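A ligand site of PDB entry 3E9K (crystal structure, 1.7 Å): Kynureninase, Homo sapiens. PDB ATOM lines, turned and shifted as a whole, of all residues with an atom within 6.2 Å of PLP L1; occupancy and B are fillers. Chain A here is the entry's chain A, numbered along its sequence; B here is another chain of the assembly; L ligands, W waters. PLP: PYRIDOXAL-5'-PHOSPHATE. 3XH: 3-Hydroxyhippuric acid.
C4A of PLP L1 is covalently linked to NZ of Lys 276 (1.4 Å).
The side-chain hydroxyl of Ser 332 of chain B lies within hydrogen-bond range of an oxygen (O1P) of PLP L1 (2.6 Å).
OD2 of Asp 168 is in hydrogen-bond range of N1 of PLP L1, 2.7 Å away.
O2P of PLP L1 lies within hydrogen-bond range of OH of Tyr 275, at 2.7 Å.
The backbone NH (N) of Thr 138 lies within hydrogen-bond range of an oxygen (O1P) of PLP L1 (2.9 Å).
The side-chain hydroxyl (OG1) of Thr 138 lies within hydrogen-bond range of an oxygen (O1P) of PLP L1 (2.8 Å).
An oxygen (O3P) of PLP L1 lies within hydrogen-bond range of the indole nitrogen (NE1) of Trp 305 of chain B, at 2.8 Å.
The backbone NH of Asn 333 of chain B sits at hydrogen-bond distance from an oxygen (O3P) of PLP L1 (3.0 Å).
An oxygen (O3P) of PLP L1 is in hydrogen-bond range of the side-chain amide nitrogen (ND2) of Asn 333 of chain B (2.8 Å).
NE2 of His 253 lies close to O3 of PLP L1, at 3.4 Å.
O14 of 3XH L2 lies close to NZ of Lys 276 (3.4 Å).
A ring nitrogen (NE2) of His 253 lies within hydrogen-bond range of an oxygen (O12) of 3XH L2 (2.8 Å).
The side-chain carboxylate of Asp 250 lies close to the side-chain carboxylate of Asp 168 (2.5 Å).
The side-chain hydroxyl (OH) of Tyr 275 lies within hydrogen-bond range of the side-chain amide nitrogen (ND2) of Asn 333 of chain B (3.1 Å).
The side-chain hydroxyl (OG) of Ser 167 lies within hydrogen-bond range of the side-chain hydroxyl (OG1) of Thr 138.
The backbone NH (N) of Trp 305 of chain B is in hydrogen-bond range of the side-chain hydroxyl (OG) of Ser 167, at 3.0 Å.
The backbone carbonyl oxygen of Ile 331 of chain B is in hydrogen-bond range of the backbone NH of Trp 305 of chain B.
N of Ala 252 lies within hydrogen-bond range of OD1 of Asp 250, at 2.9 Å.
N1 of PLP L1 sits close to OD2 of Asp 250.
Leu 137 touches PLP L1 (CD2 to C6, 3.5 Å).
Phe 165 touches PLP L1.
Ala 252 touches PLP L1.
Hydrophobic or aromatic side chains that line PLP L1: Leu 137, Phe 165, Ala 252, His 253, Tyr 275 and Trp 305 of chain B.
Along chain A the residues within 4 Å of PLP L1 span positions 137 to 276.
The nearest printed residue that does not touch PLP L1 is Ser 167 (4.1 Å).
Water W1 lies within hydrogen-bond range of an oxygen (O2P) of PLP L1 (2.6 Å) and the backbone NH of Leu 137 (2.8 Å).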
ATOM      1  N   ALA A 136      18.389  12.479  20.261  1.00  0.00           N
ATOM      2  CA  ALA A 136      19.560  13.133  19.675  1.00  0.00           C
ATOM      3  C   ALA A 136      20.637  13.180  20.738  1.00  0.00           C
ATOM      4  O   ALA A 136      20.347  12.968  21.934  1.00  0.00           O
ATOM      5  CB  ALA A 136      19.199  14.534  19.207  1.00  0.00           C
ATOM      6  N   LEU A 137      21.864  13.416  20.316  1.00  0.00           N
ATOM      7  CA  LEU A 137      23.008  13.309  21.228  1.00  0.00           C
ATOM      8  C   LEU A 137      22.867  14.205  22.472  1.00  0.00           C
ATOM      9  O   LEU A 137      22.862  13.706  23.602  1.00  0.00           O
ATOM     10  CB  LEU A 137      24.308  13.602  20.473  1.00  0.00           C
ATOM     11  CG  LEU A 137      25.595  13.790  21.294  1.00  0.00           C
ATOM     12  CD1 LEU A 137      25.840  12.685  22.281  1.00  0.00           C
ATOM     13  CD2 LEU A 137      26.792  13.958  20.377  1.00  0.00           C
ATOM     14  N   THR A 138      22.746  15.503  22.259  1.00  0.00           N
ATOM     15  CA  THR A 138      22.736  16.434  23.409  1.00  0.00           C
ATOM     16  C   THR A 138      21.494  16.215  24.273  1.00  0.00           C
ATOM     17  O   THR A 138      21.547  16.354  25.494  1.00  0.00           O
ATOM     18  CB  THR A 138      22.895  17.909  22.990  1.00  0.00           C
ATOM     19  OG1 THR A 138      24.039  18.043  22.120  1.00  0.00           O
ATOM     20  CG2 THR A 138      23.115  18.767  24.247  1.00  0.00           C
ATOM     21  N   VAL A 139      20.382  15.839  23.644  1.00  0.00           N
ATOM     22  CA  VAL A 139      19.169  15.468  24.389  1.00  0.00           C
ATOM     23  C   VAL A 139      19.481  14.314  25.336  1.00  0.00           C
ATOM     24  O   VAL A 139      19.182  14.388  26.538  1.00  0.00           O
ATOM     25  CB  VAL A 139      17.981  15.117  23.449  1.00  0.00           C
ATOM     26  CG1 VAL A 139      16.748  14.658  24.237  1.00  0.00           C
ATOM     27  CG2 VAL A 139      17.594  16.334  22.591  1.00  0.00           C
ATOM     28  N   PHE A 165      33.084  20.800  23.033  1.00  0.00           N
ATOM     29  CA  PHE A 165      32.113  21.112  21.986  1.00  0.00           C
ATOM     30  C   PHE A 165      31.022  22.016  22.575  1.00  0.00           C
ATOM     31  O   PHE A 165      30.637  21.824  23.726  1.00  0.00           O
ATOM     32  CB  PHE A 165      31.521  19.826  21.411  1.00  0.00           C
ATOM     33  CG  PHE A 165      30.733  20.047  20.161  1.00  0.00           C
ATOM     34  CD1 PHE A 165      31.371  20.156  18.938  1.00  0.00           C
ATOM     35  CD2 PHE A 165      29.348  20.202  20.202  1.00  0.00           C
ATOM     36  CE1 PHE A 165      30.656  20.404  17.770  1.00  0.00           C
ATOM     37  CE2 PHE A 165      28.619  20.435  19.040  1.00  0.00           C
ATOM     38  CZ  PHE A 165      29.271  20.541  17.828  1.00  0.00           C
ATOM     39  N   SER A 167      27.809  22.395  22.320  1.00  0.00           N
ATOM     40  CA  SER A 167      26.558  21.813  22.823  1.00  0.00           C
ATOM     41  C   SER A 167      26.732  21.234  24.224  1.00  0.00           C
ATOM     42  O   SER A 167      25.900  21.466  25.107  1.00  0.00           O
ATOM     43  CB  SER A 167      25.998  20.757  21.868  1.00  0.00           C
ATOM     44  OG  SER A 167      24.594  20.614  22.057  1.00  0.00           O
ATOM     45  N   ASP A 168      27.839  20.498  24.425  1.00  0.00           N
ATOM     46  CA  ASP A 168      28.165  19.900  25.718  1.00  0.00           C
ATOM     47  C   ASP A 168      28.407  20.970  26.772  1.00  0.00           C
ATOM     48  O   ASP A 168      27.962  20.860  27.909  1.00  0.00           O
ATOM     49  CB  ASP A 168      29.413  19.036  25.593  1.00  0.00           C
ATOM     50  CG  ASP A 168      29.222  17.876  24.652  1.00  0.00           C
ATOM     51  OD1 ASP A 168      29.288  16.724  25.115  1.00  0.00           O
ATOM     52  OD2 ASP A 168      28.957  18.118  23.459  1.00  0.00           O
ATOM     53  N   SER A 221      34.870  14.364  26.480  1.00  0.00           N
ATOM     54  CA  SER A 221      34.730  13.761  25.172  1.00  0.00           C
ATOM     55  C   SER A 221      35.667  12.548  25.125  1.00  0.00           C
ATOM     56  O   SER A 221      36.680  12.503  25.853  1.00  0.00           O
ATOM     57  CB  SER A 221      35.048  14.756  24.061  1.00  0.00           C
ATOM     58  OG  SER A 221      36.339  15.297  24.239  1.00  0.00           O
ATOM     59  N   VAL A 223      36.872  11.557  22.055  1.00  0.00           N
ATOM     60  CA  VAL A 223      37.783  12.197  21.097  1.00  0.00           C
ATOM     61  C   VAL A 223      37.398  13.664  21.021  1.00  0.00           C
ATOM     62  O   VAL A 223      36.213  14.003  20.858  1.00  0.00           O
ATOM     63  CB  VAL A 223      37.699  11.542  19.686  1.00  0.00           C
ATOM     64  CG1 VAL A 223      38.504  12.319  18.665  1.00  0.00           C
ATOM     65  CG2 VAL A 223      38.168  10.076  19.746  1.00  0.00           C
ATOM     66  N   PHE A 225      36.778  17.083  19.396  1.00  0.00           N
ATOM     67  CA  PHE A 225      36.359  17.452  18.040  1.00  0.00           C
ATOM     68  C   PHE A 225      37.357  18.333  17.300  1.00  0.00           C
ATOM     69  O   PHE A 225      37.489  18.227  16.077  1.00  0.00           O
ATOM     70  CB  PHE A 225      34.972  18.118  18.051  1.00  0.00           C
ATOM     71  CG  PHE A 225      34.981  19.559  18.481  1.00  0.00           C
ATOM     72  CD1 PHE A 225      35.201  19.906  19.810  1.00  0.00           C
ATOM     73  CD2 PHE A 225      34.753  20.577  17.555  1.00  0.00           C
ATOM     74  CE1 PHE A 225      35.214  21.246  20.211  1.00  0.00           C
ATOM     75  CE2 PHE A 225      34.752  21.918  17.946  1.00  0.00           C
ATOM     76  CZ  PHE A 225      34.989  22.252  19.279  1.00  0.00           C
ATOM     77  N   ASP A 250      31.050  11.883  26.191  1.00  0.00           N
ATOM     78  CA  ASP A 250      30.429  12.165  24.910  1.00  0.00           C
ATOM     79  C   ASP A 250      31.312  11.536  23.834  1.00  0.00           C
ATOM     80  O   ASP A 250      32.421  12.013  23.547  1.00  0.00           O
ATOM     81  CB  ASP A 250      30.272  13.668  24.670  1.00  0.00           C
ATOM     82  CG  ASP A 250      29.544  13.985  23.372  1.00  0.00           C
ATOM     83  OD1 ASP A 250      29.587  13.145  22.454  1.00  0.00           O
ATOM     84  OD2 ASP A 250      28.926  15.069  23.254  1.00  0.00           O
ATOM     85  N   ALA A 252      30.772  11.224  20.570  1.00  0.00           N
ATOM     86  CA  ALA A 252      30.416  11.708  19.224  1.00  0.00           C
ATOM     87  C   ALA A 252      31.500  11.436  18.192  1.00  0.00           C
ATOM     88  O   ALA A 252      31.215  11.008  17.075  1.00  0.00           O
ATOM     89  CB  ALA A 252      30.114  13.195  19.263  1.00  0.00           C
ATOM     90  N   HIS A 253      32.752  11.702  18.584  1.00  0.00           N
ATOM     91  CA  HIS A 253      33.881  11.516  17.679  1.00  0.00           C
ATOM     92  C   HIS A 253      34.633  10.213  17.887  1.00  0.00           C
ATOM     93  O   HIS A 253      35.650   9.970  17.231  1.00  0.00           O
ATOM     94  CB  HIS A 253      34.827  12.712  17.754  1.00  0.00           C
ATOM     95  CG  HIS A 253      34.390  13.876  16.918  1.00  0.00           C
ATOM     96  ND1 HIS A 253      34.775  14.040  15.606  1.00  0.00           N
ATOM     97  CD2 HIS A 253      33.559  14.904  17.203  1.00  0.00           C
ATOM     98  CE1 HIS A 253      34.217  15.140  15.117  1.00  0.00           C
ATOM     99  NE2 HIS A 253      33.468  15.678  16.068  1.00  0.00           N
ATOM    100  N   CYS A 273      26.315  10.470  18.793  1.00  0.00           N
ATOM    101  CA  CYS A 273      25.471  10.740  17.636  1.00  0.00           C
ATOM    102  C   CYS A 273      25.726   9.667  16.573  1.00  0.00           C
ATOM    103  O   CYS A 273      26.685   8.900  16.688  1.00  0.00           O
ATOM    104  CB  CYS A 273      25.764  12.121  17.082  1.00  0.00           C
ATOM    105  SG  CYS A 273      27.495  12.329  16.628  1.00  0.00           S
ATOM    106  N   TYR A 275      25.516  10.333  12.958  1.00  0.00           N
ATOM    107  CA  TYR A 275      25.675  10.887  11.619  1.00  0.00           C
ATOM    108  C   TYR A 275      27.107  11.244  11.258  1.00  0.00           C
ATOM    109  O   TYR A 275      27.364  11.737  10.157  1.00  0.00           O
ATOM    110  CB  TYR A 275      24.740  12.103  11.420  1.00  0.00           C
ATOM    111  CG  TYR A 275      24.920  13.150  12.497  1.00  0.00           C
ATOM    112  CD1 TYR A 275      25.964  14.074  12.439  1.00  0.00           C
ATOM    113  CD2 TYR A 275      24.067  13.179  13.611  1.00  0.00           C
ATOM    114  CE1 TYR A 275      26.150  15.020  13.445  1.00  0.00           C
ATOM    115  CE2 TYR A 275      24.234  14.118  14.620  1.00  0.00           C
ATOM    116  CZ  TYR A 275      25.273  15.040  14.531  1.00  0.00           C
ATOM    117  OH  TYR A 275      25.452  15.967  15.522  1.00  0.00           O
ATOM    118  N   LYS A 276      28.027  10.997  12.190  1.00  0.00           N
ATOM    119  CA  LYS A 276      29.414  11.211  11.956  1.00  0.00           C
ATOM    120  C   LYS A 276      30.032   9.903  11.411  1.00  0.00           C
ATOM    121  O   LYS A 276      29.725   9.543  10.324  1.00  0.00           O
ATOM    122  CB  LYS A 276      30.117  11.718  13.222  1.00  0.00           C
ATOM    123  CG  LYS A 276      29.625  13.062  13.652  1.00  0.00           C
ATOM    124  CD  LYS A 276      30.210  13.679  14.897  1.00  0.00           C
ATOM    125  CE  LYS A 276      29.748  15.095  15.034  1.00  0.00           C
ATOM    126  NZ  LYS A 276      29.720  15.770  16.318  1.00  0.00           N
ATOM    127  N   TRP B 305      23.351  23.306  21.584  1.00  0.00           N
ATOM    128  CA  TRP B 305      23.835  24.263  20.604  1.00  0.00           C
ATOM    129  C   TRP B 305      22.791  24.735  19.590  1.00  0.00           C
ATOM    130  O   TRP B 305      22.932  25.820  19.032  1.00  0.00           O
ATOM    131  CB  TRP B 305      25.129  23.803  19.932  1.00  0.00           C
ATOM    132  CG  TRP B 305      25.017  22.671  18.956  1.00  0.00           C
ATOM    133  CD1 TRP B 305      24.257  21.541  19.058  1.00  0.00           C
ATOM    134  CD2 TRP B 305      25.745  22.567  17.728  1.00  0.00           C
ATOM    135  NE1 TRP B 305      24.472  20.725  17.951  1.00  0.00           N
ATOM    136  CE2 TRP B 305      25.374  21.346  17.127  1.00  0.00           C
ATOM    137  CE3 TRP B 305      26.673  23.397  17.083  1.00  0.00           C
ATOM    138  CZ2 TRP B 305      25.909  20.935  15.890  1.00  0.00           C
ATOM    139  CZ3 TRP B 305      27.200  22.986  15.858  1.00  0.00           C
ATOM    140  CH2 TRP B 305      26.812  21.764  15.280  1.00  0.00           C
ATOM    141  N   PHE B 306      21.739  23.949  19.367  1.00  0.00           N
ATOM    142  CA  PHE B 306      20.715  24.404  18.411  1.00  0.00           C
ATOM    143  C   PHE B 306      19.704  25.403  18.993  1.00  0.00           C
ATOM    144  O   PHE B 306      18.771  25.823  18.298  1.00  0.00           O
ATOM    145  CB  PHE B 306      20.079  23.233  17.649  1.00  0.00           C
ATOM    146  CG  PHE B 306      20.724  22.985  16.317  1.00  0.00           C
ATOM    147  CD1 PHE B 306      22.082  22.666  16.240  1.00  0.00           C
ATOM    148  CD2 PHE B 306      19.999  23.145  15.138  1.00  0.00           C
ATOM    149  CE1 PHE B 306      22.702  22.469  14.997  1.00  0.00           C
ATOM    150  CE2 PHE B 306      20.610  22.941  13.888  1.00  0.00           C
ATOM    151  CZ  PHE B 306      21.964  22.613  13.825  1.00  0.00           C
ATOM    152  N   ILE B 331      17.381  21.642  21.246  1.00  0.00           N
ATOM    153  CA  ILE B 331      18.663  21.245  21.805  1.00  0.00           C
ATOM    154  C   ILE B 331      19.642  20.798  20.714  1.00  0.00           C
ATOM    155  O   ILE B 331      20.794  21.251  20.686  1.00  0.00           O
ATOM    156  CB  ILE B 331      18.442  20.137  22.886  1.00  0.00           C
ATOM    157  CG1 ILE B 331      17.744  20.741  24.107  1.00  0.00           C
ATOM    158  CG2 ILE B 331      19.772  19.490  23.275  1.00  0.00           C
ATOM    159  CD1 ILE B 331      17.257  19.725  25.161  1.00  0.00           C
ATOM    160  N   SER B 332      19.173  19.940  19.801  1.00  0.00           N
ATOM    161  CA  SER B 332      20.046  19.243  18.856  1.00  0.00           C
ATOM    162  C   SER B 332      19.704  19.539  17.404  1.00  0.00           C
ATOM    163  O   SER B 332      18.620  20.069  17.105  1.00  0.00           O
ATOM    164  CB  SER B 332      19.970  17.721  19.106  1.00  0.00           C
ATOM    165  OG  SER B 332      20.488  17.426  20.398  1.00  0.00           O
ATOM    166  N   ASN B 333      20.626  19.218  16.505  1.00  0.00           N
ATOM    167  CA  ASN B 333      20.374  19.389  15.071  1.00  0.00           C
ATOM    168  C   ASN B 333      19.212  18.484  14.609  1.00  0.00           C
ATOM    169  O   ASN B 333      19.080  17.350  15.109  1.00  0.00           O
ATOM    170  CB  ASN B 333      21.662  19.159  14.255  1.00  0.00           C
ATOM    171  CG  ASN B 333      22.030  17.695  14.151  1.00  0.00           C
ATOM    172  OD1 ASN B 333      21.852  17.076  13.105  1.00  0.00           O
ATOM    173  ND2 ASN B 333      22.563  17.137  15.247  1.00  0.00           N
HETATM  174  N1  PLP L   1      28.760  17.070  21.026  1.00  0.00           N
HETATM  175  C2  PLP L   1      29.904  16.639  20.385  1.00  0.00           C
HETATM  176  C2A PLP L   1      31.134  16.331  21.192  1.00  0.00           C
HETATM  177  C3  PLP L   1      29.914  16.482  19.007  1.00  0.00           C
HETATM  178  O3  PLP L   1      31.077  16.165  18.367  1.00  0.00           O
HETATM  179  C4  PLP L   1      28.777  16.767  18.276  1.00  0.00           C
HETATM  180  C4A PLP L   1      28.797  16.656  16.775  1.00  0.00           C
HETATM  181  C5  PLP L   1      27.620  17.202  18.916  1.00  0.00           C
HETATM  182  C6  PLP L   1      27.623  17.355  20.295  1.00  0.00           C
HETATM  183  C5A PLP L   1      26.373  17.506  18.122  1.00  0.00           C
HETATM  184  O4P PLP L   1      25.287  17.681  18.997  1.00  0.00           O
HETATM  185  P   PLP L   1      23.809  17.202  18.576  1.00  0.00           P
HETATM  186  O1P PLP L   1      22.977  16.954  19.806  1.00  0.00           O
HETATM  187  O2P PLP L   1      23.905  15.923  17.765  1.00  0.00           O
HETATM  188  O3P PLP L   1      23.175  18.280  17.739  1.00  0.00           O
HETATM  189  O11 3XH L   2      31.829  18.011  12.975  1.00  0.00           O
HETATM  190  C10 3XH L   2      31.875  18.294  14.189  1.00  0.00           C
HETATM  191  O12 3XH L   2      32.878  18.114  14.912  1.00  0.00           O
HETATM  192  C9  3XH L   2      30.668  18.907  14.844  1.00  0.00           C
HETATM  193  N8  3XH L   2      29.681  19.404  13.892  1.00  0.00           N
HETATM  194  C7  3XH L   2      28.546  18.805  13.545  1.00  0.00           C
HETATM  195  O14 3XH L   2      28.205  17.735  14.025  1.00  0.00           O
HETATM  196  C6  3XH L   2      27.644  19.488  12.576  1.00  0.00           C
HETATM  197  C5  3XH L   2      28.130  20.271  11.519  1.00  0.00           C
HETATM  198  C4  3XH L   2      27.238  20.900  10.653  1.00  0.00           C
HETATM  199  C3  3XH L   2      25.871  20.775  10.844  1.00  0.00           C
HETATM  200  C2  3XH L   2      25.381  20.005  11.907  1.00  0.00           C
HETATM  201  O13 3XH L   2      24.045  19.869  12.121  1.00  0.00           O
HETATM  202  C1  3XH L   2      26.263  19.368  12.766  1.00  0.00           C
HETATM  203  O   HOH W   1      22.325  13.917  17.619  1.00  0.00           O
